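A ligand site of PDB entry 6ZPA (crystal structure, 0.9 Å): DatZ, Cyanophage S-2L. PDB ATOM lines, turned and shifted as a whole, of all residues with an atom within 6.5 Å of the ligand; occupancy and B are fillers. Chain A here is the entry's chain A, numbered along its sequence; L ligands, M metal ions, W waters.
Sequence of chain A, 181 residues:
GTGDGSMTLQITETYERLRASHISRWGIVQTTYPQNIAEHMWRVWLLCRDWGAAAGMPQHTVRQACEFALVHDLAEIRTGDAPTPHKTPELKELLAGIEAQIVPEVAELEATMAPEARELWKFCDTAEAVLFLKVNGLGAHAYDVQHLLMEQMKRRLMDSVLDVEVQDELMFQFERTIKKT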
ATOM      1  N   SER A  24      37.948  24.019  -0.853  1.00  0.00           N
ATOM      2  CA  SER A  24      37.794  24.026  -2.302  1.00  0.00           C
ATOM      3  C   SER A  24      36.402  23.546  -2.724  1.00  0.00           C
ATOM      4  O   SER A  24      35.930  22.491  -2.264  1.00  0.00           O
ATOM      5  CB  SER A  24      38.848  23.130  -2.950  1.00  0.00           C
ATOM      6  OG  SER A  24      40.161  23.568  -2.661  1.00  0.00           O
ATOM      7  N   ARG A  25      35.797  24.303  -3.626  1.00  0.00           N
ATOM      8  CA  ARG A  25      34.535  23.964  -4.258  1.00  0.00           C
ATOM      9  C   ARG A  25      34.774  23.078  -5.484  1.00  0.00           C
ATOM     10  O   ARG A  25      35.909  22.805  -5.881  1.00  0.00           O
ATOM     11  CB  ARG A  25      33.789  25.251  -4.626  1.00  0.00           C
ATOM     12  CG  ARG A  25      33.231  25.946  -3.400  1.00  0.00           C
ATOM     13  CD  ARG A  25      32.760  27.358  -3.701  1.00  0.00           C
ATOM     14  NE  ARG A  25      31.807  27.446  -4.821  1.00  0.00           N
ATOM     15  CZ  ARG A  25      30.499  27.215  -4.746  1.00  0.00           C
ATOM     16  NH1 ARG A  25      29.938  26.856  -3.602  1.00  0.00           N
ATOM     17  NH2 ARG A  25      29.753  27.354  -5.829  1.00  0.00           N
ATOM     18  N   TRP A  26      33.677  22.613  -6.100  1.00  0.00           N
ATOM     19  CA  TRP A  26      33.753  21.893  -7.379  1.00  0.00           C
ATOM     20  C   TRP A  26      34.553  20.602  -7.253  1.00  0.00           C
ATOM     21  O   TRP A  26      35.248  20.194  -8.182  1.00  0.00           O
ATOM     22  CB  TRP A  26      34.281  22.768  -8.508  1.00  0.00           C
ATOM     23  CG  TRP A  26      33.480  24.008  -8.662  1.00  0.00           C
ATOM     24  CD1 TRP A  26      33.852  25.276  -8.316  1.00  0.00           C
ATOM     25  CD2 TRP A  26      32.132  24.087  -9.122  1.00  0.00           C
ATOM     26  NE1 TRP A  26      32.811  26.148  -8.544  1.00  0.00           N
ATOM     27  CE2 TRP A  26      31.748  25.448  -9.054  1.00  0.00           C
ATOM     28  CE3 TRP A  26      31.215  23.142  -9.611  1.00  0.00           C
ATOM     29  CZ2 TRP A  26      30.487  25.890  -9.476  1.00  0.00           C
ATOM     30  CZ3 TRP A  26      29.971  23.582 -10.008  1.00  0.00           C
ATOM     31  CH2 TRP A  26      29.624  24.940  -9.942  1.00  0.00           C
ATOM     32  N   GLY A  27      34.388  19.895  -6.145  1.00  0.00           N
ATOM     33  CA  GLY A  27      35.169  18.696  -5.923  1.00  0.00           C
ATOM     34  C   GLY A  27      34.926  17.552  -6.894  1.00  0.00           C
ATOM     35  O   GLY A  27      35.729  16.624  -6.906  1.00  0.00           O
ATOM     36  N   ILE A  28      33.839  17.569  -7.668  1.00  0.00           N
ATOM     37  CA  ILE A  28      33.608  16.524  -8.667  1.00  0.00           C
ATOM     38  C   ILE A  28      33.580  17.061 -10.094  1.00  0.00           C
ATOM     39  O   ILE A  28      33.226  16.328 -11.026  1.00  0.00           O
ATOM     40  CB  ILE A  28      32.377  15.632  -8.364  1.00  0.00           C
ATOM     41  CG1 ILE A  28      31.043  16.350  -8.597  1.00  0.00           C
ATOM     42  CG2 ILE A  28      32.478  15.068  -6.955  1.00  0.00           C
ATOM     43  CD1 ILE A  28      29.871  15.385  -8.657  1.00  0.00           C
ATOM     44  N   VAL A  29      33.977  18.321 -10.294  1.00  0.00           N
ATOM     45  CA  VAL A  29      33.920  18.980 -11.590  1.00  0.00           C
ATOM     46  C   VAL A  29      35.299  19.538 -11.942  1.00  0.00           C
ATOM     47  O   VAL A  29      35.934  20.205 -11.114  1.00  0.00           O
ATOM     48  CB  VAL A  29      32.886  20.131 -11.576  1.00  0.00           C
ATOM     49  CG1 VAL A  29      32.856  20.838 -12.926  1.00  0.00           C
ATOM     50  CG2 VAL A  29      31.509  19.613 -11.210  1.00  0.00           C
ATOM     51  N   GLN A  35      38.499  26.891  -6.829  1.00  0.00           N
ATOM     52  CA  GLN A  35      37.837  28.032  -6.206  1.00  0.00           C
ATOM     53  C   GLN A  35      37.594  27.721  -4.732  1.00  0.00           C
ATOM     54  O   GLN A  35      37.150  26.624  -4.397  1.00  0.00           O
ATOM     55  CB  GLN A  35      36.474  28.255  -6.869  1.00  0.00           C
ATOM     56  CG  GLN A  35      35.829  29.556  -6.459  1.00  0.00           C
ATOM     57  CD  GLN A  35      34.370  29.665  -6.821  1.00  0.00           C
ATOM     58  OE1 GLN A  35      33.638  28.659  -6.876  1.00  0.00           O
ATOM     59  NE2 GLN A  35      33.919  30.894  -7.025  1.00  0.00           N
ATOM     60  N   HIS A  40      33.891  32.591  -3.189  1.00  0.00           N
ATOM     61  CA  HIS A  40      32.478  32.313  -3.478  1.00  0.00           C
ATOM     62  C   HIS A  40      31.565  33.184  -2.625  1.00  0.00           C
ATOM     63  O   HIS A  40      30.635  33.807  -3.143  1.00  0.00           O
ATOM     64  CB  HIS A  40      32.202  30.821  -3.274  1.00  0.00           C
ATOM     65  CG  HIS A  40      30.755  30.462  -3.118  1.00  0.00           C
ATOM     66  ND1 HIS A  40      29.845  30.454  -4.153  1.00  0.00           N
ATOM     67  CD2 HIS A  40      30.066  30.044  -2.021  1.00  0.00           C
ATOM     68  CE1 HIS A  40      28.660  30.068  -3.681  1.00  0.00           C
ATOM     69  NE2 HIS A  40      28.764  29.817  -2.402  1.00  0.00           N
ATOM     70  N   ASP A  73      28.368  29.347   4.085  1.00  0.00           N
ATOM     71  CA  ASP A  73      29.081  28.098   3.841  1.00  0.00           C
ATOM     72  C   ASP A  73      30.171  27.827   4.880  1.00  0.00           C
ATOM     73  O   ASP A  73      30.973  26.911   4.683  1.00  0.00           O
ATOM     74  CB  ASP A  73      29.628  28.049   2.411  1.00  0.00           C
ATOM     75  CG  ASP A  73      28.541  27.747   1.375  1.00  0.00           C
ATOM     76  OD1 ASP A  73      27.531  27.094   1.743  1.00  0.00           O
ATOM     77  OD2 ASP A  73      28.694  28.154   0.202  1.00  0.00           O
ATOM     78  N   GLU A  76      31.438  24.325   6.024  1.00  0.00           N
ATOM     79  CA  GLU A  76      32.263  23.523   5.129  1.00  0.00           C
ATOM     80  C   GLU A  76      33.724  23.514   5.548  1.00  0.00           C
ATOM     81  O   GLU A  76      34.474  22.655   5.093  1.00  0.00           O
ATOM     82  CB  GLU A  76      32.095  24.013   3.689  1.00  0.00           C
ATOM     83  CG  GLU A  76      30.680  23.817   3.171  1.00  0.00           C
ATOM     84  CD  GLU A  76      30.480  24.300   1.755  1.00  0.00           C
ATOM     85  OE1 GLU A  76      31.364  24.995   1.233  1.00  0.00           O
ATOM     86  OE2 GLU A  76      29.430  23.980   1.153  1.00  0.00           O
ATOM     87  N   ASP A  81      32.886  20.888   1.123  1.00  0.00           N
ATOM     88  CA  ASP A  81      31.839  21.254   0.196  1.00  0.00           C
ATOM     89  C   ASP A  81      31.463  19.990  -0.572  1.00  0.00           C
ATOM     90  O   ASP A  81      32.341  19.300  -1.110  1.00  0.00           O
ATOM     91  CB  ASP A  81      32.359  22.338  -0.736  1.00  0.00           C
ATOM     92  CG  ASP A  81      31.487  22.540  -1.944  1.00  0.00           C
ATOM     93  OD1 ASP A  81      30.402  23.141  -1.785  1.00  0.00           O
ATOM     94  OD2 ASP A  81      31.868  22.072  -3.031  1.00  0.00           O
ATOM     95  N   ALA A  82      30.181  19.647  -0.564  1.00  0.00           N
ATOM     96  CA  ALA A  82      29.695  18.452  -1.220  1.00  0.00           C
ATOM     97  C   ALA A  82      28.862  18.821  -2.445  1.00  0.00           C
ATOM     98  O   ALA A  82      28.227  19.874  -2.474  1.00  0.00           O
ATOM     99  CB  ALA A  82      28.823  17.641  -0.253  1.00  0.00           C
ATOM    100  N   PRO A  83      28.838  17.968  -3.458  1.00  0.00           N
ATOM    101  CA  PRO A  83      28.160  18.343  -4.712  1.00  0.00           C
ATOM    102  C   PRO A  83      26.665  18.390  -4.550  1.00  0.00           C
ATOM    103  O   PRO A  83      26.056  17.527  -3.910  1.00  0.00           O
ATOM    104  CB  PRO A  83      28.557  17.219  -5.686  1.00  0.00           C
ATOM    105  CG  PRO A  83      29.592  16.424  -5.009  1.00  0.00           C
ATOM    106  CD  PRO A  83      29.510  16.661  -3.551  1.00  0.00           C
ATOM    107  N   THR A  84      26.045  19.377  -5.198  1.00  0.00           N
ATOM    108  CA  THR A  84      24.594  19.551  -5.110  1.00  0.00           C
ATOM    109  C   THR A  84      23.804  18.261  -5.357  1.00  0.00           C
ATOM    110  O   THR A  84      22.897  17.967  -4.562  1.00  0.00           O
ATOM    111  CB  THR A  84      24.166  20.684  -6.053  1.00  0.00           C
ATOM    112  OG1 THR A  84      24.906  21.857  -5.741  1.00  0.00           O
ATOM    113  CG2 THR A  84      22.673  20.962  -5.914  1.00  0.00           C
ATOM    114  N   PRO A  85      24.072  17.481  -6.409  1.00  0.00           N
ATOM    115  CA  PRO A  85      23.233  16.286  -6.649  1.00  0.00           C
ATOM    116  C   PRO A  85      23.289  15.277  -5.530  1.00  0.00           C
ATOM    117  O   PRO A  85      22.344  14.499  -5.345  1.00  0.00           O
ATOM    118  CB  PRO A  85      23.773  15.714  -7.963  1.00  0.00           C
ATOM    119  CG  PRO A  85      24.546  16.813  -8.595  1.00  0.00           C
ATOM    120  CD  PRO A  85      25.083  17.647  -7.467  1.00  0.00           C
ATOM    121  N   LYS A  87      23.379  15.995  -2.322  1.00  0.00           N
ATOM    122  CA  LYS A  87      22.665  16.483  -1.146  1.00  0.00           C
ATOM    123  C   LYS A  87      21.178  16.180  -1.282  1.00  0.00           C
ATOM    124  O   LYS A  87      20.346  17.053  -1.566  1.00  0.00           O
ATOM    125  CB  LYS A  87      22.900  17.976  -0.956  1.00  0.00           C
ATOM    126  CG  LYS A  87      24.335  18.363  -0.699  1.00  0.00           C
ATOM    127  CD  LYS A  87      24.416  19.860  -0.531  1.00  0.00           C
ATOM    128  CE  LYS A  87      25.829  20.340  -0.313  1.00  0.00           C
ATOM    129  NZ  LYS A  87      25.893  21.820  -0.283  1.00  0.00           N
ATOM    130  N   ASP A 125      23.378  32.539  -5.011  1.00  0.00           N
ATOM    131  CA  ASP A 125      24.305  31.446  -4.741  1.00  0.00           C
ATOM    132  C   ASP A 125      24.466  30.558  -5.971  1.00  0.00           C
ATOM    133  O   ASP A 125      25.586  30.166  -6.340  1.00  0.00           O
ATOM    134  CB  ASP A 125      23.782  30.641  -3.546  1.00  0.00           C
ATOM    135  CG  ASP A 125      24.752  29.583  -3.092  1.00  0.00           C
ATOM    136  OD1 ASP A 125      25.807  29.942  -2.553  1.00  0.00           O
ATOM    137  OD2 ASP A 125      24.474  28.395  -3.289  1.00  0.00           O
ATOM    138  N   ALA A 129      27.662  30.308  -9.128  1.00  0.00           N
ATOM    139  CA  ALA A 129      28.247  29.052  -9.590  1.00  0.00           C
ATOM    140  C   ALA A 129      28.192  28.939 -11.111  1.00  0.00           C
ATOM    141  O   ALA A 129      29.168  28.523 -11.750  1.00  0.00           O
ATOM    142  CB  ALA A 129      27.498  27.890  -8.918  1.00  0.00           C
ATOM    143  N   HIS A 141      31.251  17.523 -18.984  1.00  0.00           N
ATOM    144  CA  HIS A 141      30.512  17.400 -17.737  1.00  0.00           C
ATOM    145  C   HIS A 141      30.354  18.775 -17.073  1.00  0.00           C
ATOM    146  O   HIS A 141      29.253  19.145 -16.643  1.00  0.00           O
ATOM    147  CB  HIS A 141      31.246  16.411 -16.837  1.00  0.00           C
ATOM    148  CG  HIS A 141      30.727  16.337 -15.439  1.00  0.00           C
ATOM    149  ND1 HIS A 141      31.542  16.553 -14.354  1.00  0.00           N
ATOM    150  CD2 HIS A 141      29.487  16.056 -14.968  1.00  0.00           C
ATOM    151  CE1 HIS A 141      30.815  16.411 -13.256  1.00  0.00           C
ATOM    152  NE2 HIS A 141      29.565  16.118 -13.594  1.00  0.00           N
ATOM    153  N   ASP A 144      27.693  20.675 -18.861  1.00  0.00           N
ATOM    154  CA  ASP A 144      26.370  20.192 -18.494  1.00  0.00           C
ATOM    155  C   ASP A 144      25.965  20.700 -17.111  1.00  0.00           C
ATOM    156  O   ASP A 144      24.809  21.067 -16.904  1.00  0.00           O
ATOM    157  CB  ASP A 144      26.341  18.668 -18.492  1.00  0.00           C
ATOM    158  CG  ASP A 144      26.364  18.065 -19.871  1.00  0.00           C
ATOM    159  OD1 ASP A 144      26.186  18.803 -20.870  1.00  0.00           O
ATOM    160  OD2 ASP A 144      26.561  16.842 -19.952  1.00  0.00           O
ATOM    161  N   VAL A 145      26.899  20.686 -16.159  1.00  0.00           N
ATOM    162  CA  VAL A 145      26.604  21.164 -14.810  1.00  0.00           C
ATOM    163  C   VAL A 145      26.236  22.634 -14.833  1.00  0.00           C
ATOM    164  O   VAL A 145      25.274  23.070 -14.177  1.00  0.00           O
ATOM    165  CB  VAL A 145      27.786  20.865 -13.879  1.00  0.00           C
ATOM    166  CG1 VAL A 145      27.624  21.592 -12.549  1.00  0.00           C
ATOM    167  CG2 VAL A 145      27.937  19.353 -13.673  1.00  0.00           C
ATOM    168  N   LEU A 148      22.721  22.811 -16.190  1.00  0.00           N
ATOM    169  CA  LEU A 148      21.756  22.270 -15.245  1.00  0.00           C
ATOM    170  C   LEU A 148      21.504  23.269 -14.114  1.00  0.00           C
ATOM    171  O   LEU A 148      20.355  23.513 -13.733  1.00  0.00           O
ATOM    172  CB  LEU A 148      22.269  20.943 -14.681  1.00  0.00           C
ATOM    173  CG  LEU A 148      21.417  20.319 -13.577  1.00  0.00           C
ATOM    174  CD1 LEU A 148      20.012  20.022 -14.087  1.00  0.00           C
ATOM    175  CD2 LEU A 148      22.083  19.068 -13.035  1.00  0.00           C
ATOM    176  N   LEU A 149      22.572  23.848 -13.567  1.00  0.00           N
ATOM    177  CA  LEU A 149      22.422  24.837 -12.500  1.00  0.00           C
ATOM    178  C   LEU A 149      21.579  26.004 -12.966  1.00  0.00           C
ATOM    179  O   LEU A 149      20.726  26.509 -12.224  1.00  0.00           O
ATOM    180  CB  LEU A 149      23.791  25.329 -12.061  1.00  0.00           C
ATOM    181  CG  LEU A 149      24.533  24.368 -11.152  1.00  0.00           C
ATOM    182  CD1 LEU A 149      26.000  24.754 -11.070  1.00  0.00           C
ATOM    183  CD2 LEU A 149      23.922  24.383  -9.753  1.00  0.00           C
ATOM    184  N   GLN A 152      17.991  24.921 -12.914  1.00  0.00           N
ATOM    185  CA  GLN A 152      17.514  24.793 -11.538  1.00  0.00           C
ATOM    186  C   GLN A 152      17.254  26.157 -10.924  1.00  0.00           C
ATOM    187  O   GLN A 152      16.262  26.354 -10.214  1.00  0.00           O
ATOM    188  CB  GLN A 152      18.529  23.998 -10.721  1.00  0.00           C
ATOM    189  CG  GLN A 152      18.632  22.546 -11.150  1.00  0.00           C
ATOM    190  CD  GLN A 152      19.765  21.793 -10.481  1.00  0.00           C
ATOM    191  OE1 GLN A 152      20.776  22.378 -10.092  1.00  0.00           O
ATOM    192  NE2 GLN A 152      19.605  20.481 -10.376  1.00  0.00           N
HETATM  193  O1  LIG L   1      27.641  24.173  -3.240  1.00  0.00           O
HETATM  194  C1  LIG L   1      27.420  22.955  -3.958  1.00  0.00           C
HETATM  195  C2  LIG L   1      28.697  22.429  -4.569  1.00  0.00           C
HETATM  196  O2  LIG L   1      28.377  21.524  -5.653  1.00  0.00           O
HETATM  197  C3  LIG L   1      28.828  22.055  -6.877  1.00  0.00           C
HETATM  198  N1  LIG L   1      27.832  21.714  -7.872  1.00  0.00           N
HETATM  199  C4  LIG L   1      27.860  20.573  -8.634  1.00  0.00           C
HETATM  200  N2  LIG L   1      28.854  19.688  -8.748  1.00  0.00           N
HETATM  201  C5  LIG L   1      28.524  18.691  -9.568  1.00  0.00           C
HETATM  202  N3  LIG L   1      27.374  18.502 -10.235  1.00  0.00           N
HETATM  203  C6  LIG L   1      26.396  19.416 -10.119  1.00  0.00           C
HETATM  204  N4  LIG L   1      25.257  19.236 -10.806  1.00  0.00           N
HETATM  205  C7  LIG L   1      26.626  20.522  -9.278  1.00  0.00           C
HETATM  206  N5  LIG L   1      25.860  21.625  -8.955  1.00  0.00           N
HETATM  207  C8  LIG L   1      26.616  22.301  -8.116  1.00  0.00           C
HETATM  208  C9  LIG L   1      29.068  23.527  -6.629  1.00  0.00           C
HETATM  209  C10 LIG L   1      29.575  23.508  -5.194  1.00  0.00           C
HETATM  210  O3  LIG L   1      30.954  23.139  -5.206  1.00  0.00           O
HETATM  211 ZN    ZN M   1      27.137  28.874  -1.305  1.00  0.00          ZN
HETATM  212  O   HOH W   1      23.145  20.960  -9.675  1.00  0.00           O
HETATM  213  O   HOH W   2      31.539  19.528  -7.442  1.00  0.00           O
HETATM  214  O   HOH W   3      24.953  17.001 -12.745  1.00  0.00           O
HETATM  215  O   HOH W   4      31.387  19.740  -4.694  1.00  0.00           O
HETATM  216  O   HOH W   5      27.385  16.134 -11.743  1.00  0.00           O
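Residues that only touch the ligand: Pro 83 (3.3 Å), Ala 82 (3.3 Å), Pro 85 (3.4 Å), Leu 149 (3.5 Å), Val 145 (3.5 Å), Val 29 (3.5 Å), Arg 25 (3.6 Å), Ile 28 (3.6 Å) and Leu 148 (3.9 Å). Hydrophobic or aromatic side chains within 4 Å of the ligand: Trp 26, Ile 28, Val 29, Pro 83, Pro 85, Val 145, Leu 148 and Leu 149. Of the 24 residues printed, 12 come within 4 Å of the ligand.
The side-chain amide oxygen (OE1) of Gln 35 is in hydrogen-bond range of the indole nitrogen (NE1) of Trp 26 (3.1 Å). The guanidinium group (NH1) of Arg 25 lies close to a ring nitrogen (NE2) of His 40 (3.4 Å). N of Arg 25 lies within hydrogen-bond range of O of Gln 35, 2.8 Å away.
Water W5 lies within hydrogen-bond range of a nitrogen (N3) of the ligand (2.8 Å) and a ring nitrogen (NE2) of His 141 (2.9 Å). Water W1 lies within hydrogen-bond range of OE1 of Gln 152 (2.8 Å) and N5 of the ligand (2.9 Å). Water W2 lies within hydrogen-bond range of N2 of the ligand (3.0 Å), N of Ile 28 (3.0 Å) and N of Gly 27 (3.2 Å). Water W4 lies within hydrogen-bond range of OD2 of Asp 81 (2.9 Å), N of Gly 27 (3.3 Å) and O3 of the ligand (3.5 Å).
The side-chain carboxylate of Asp 81 sits at hydrogen-bond distance from an oxygen (O3) of the ligand. N of Trp 26 is in hydrogen-bond range of O3 of the ligand. The backbone NH (N) of Thr 84 is in hydrogen-bond range of an oxygen (O2) of the ligand (3.2 Å). A nitrogen (N5) of the ligand sits close to the side-chain hydroxyl (OG1) of Thr 84, 3.4 Å away.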
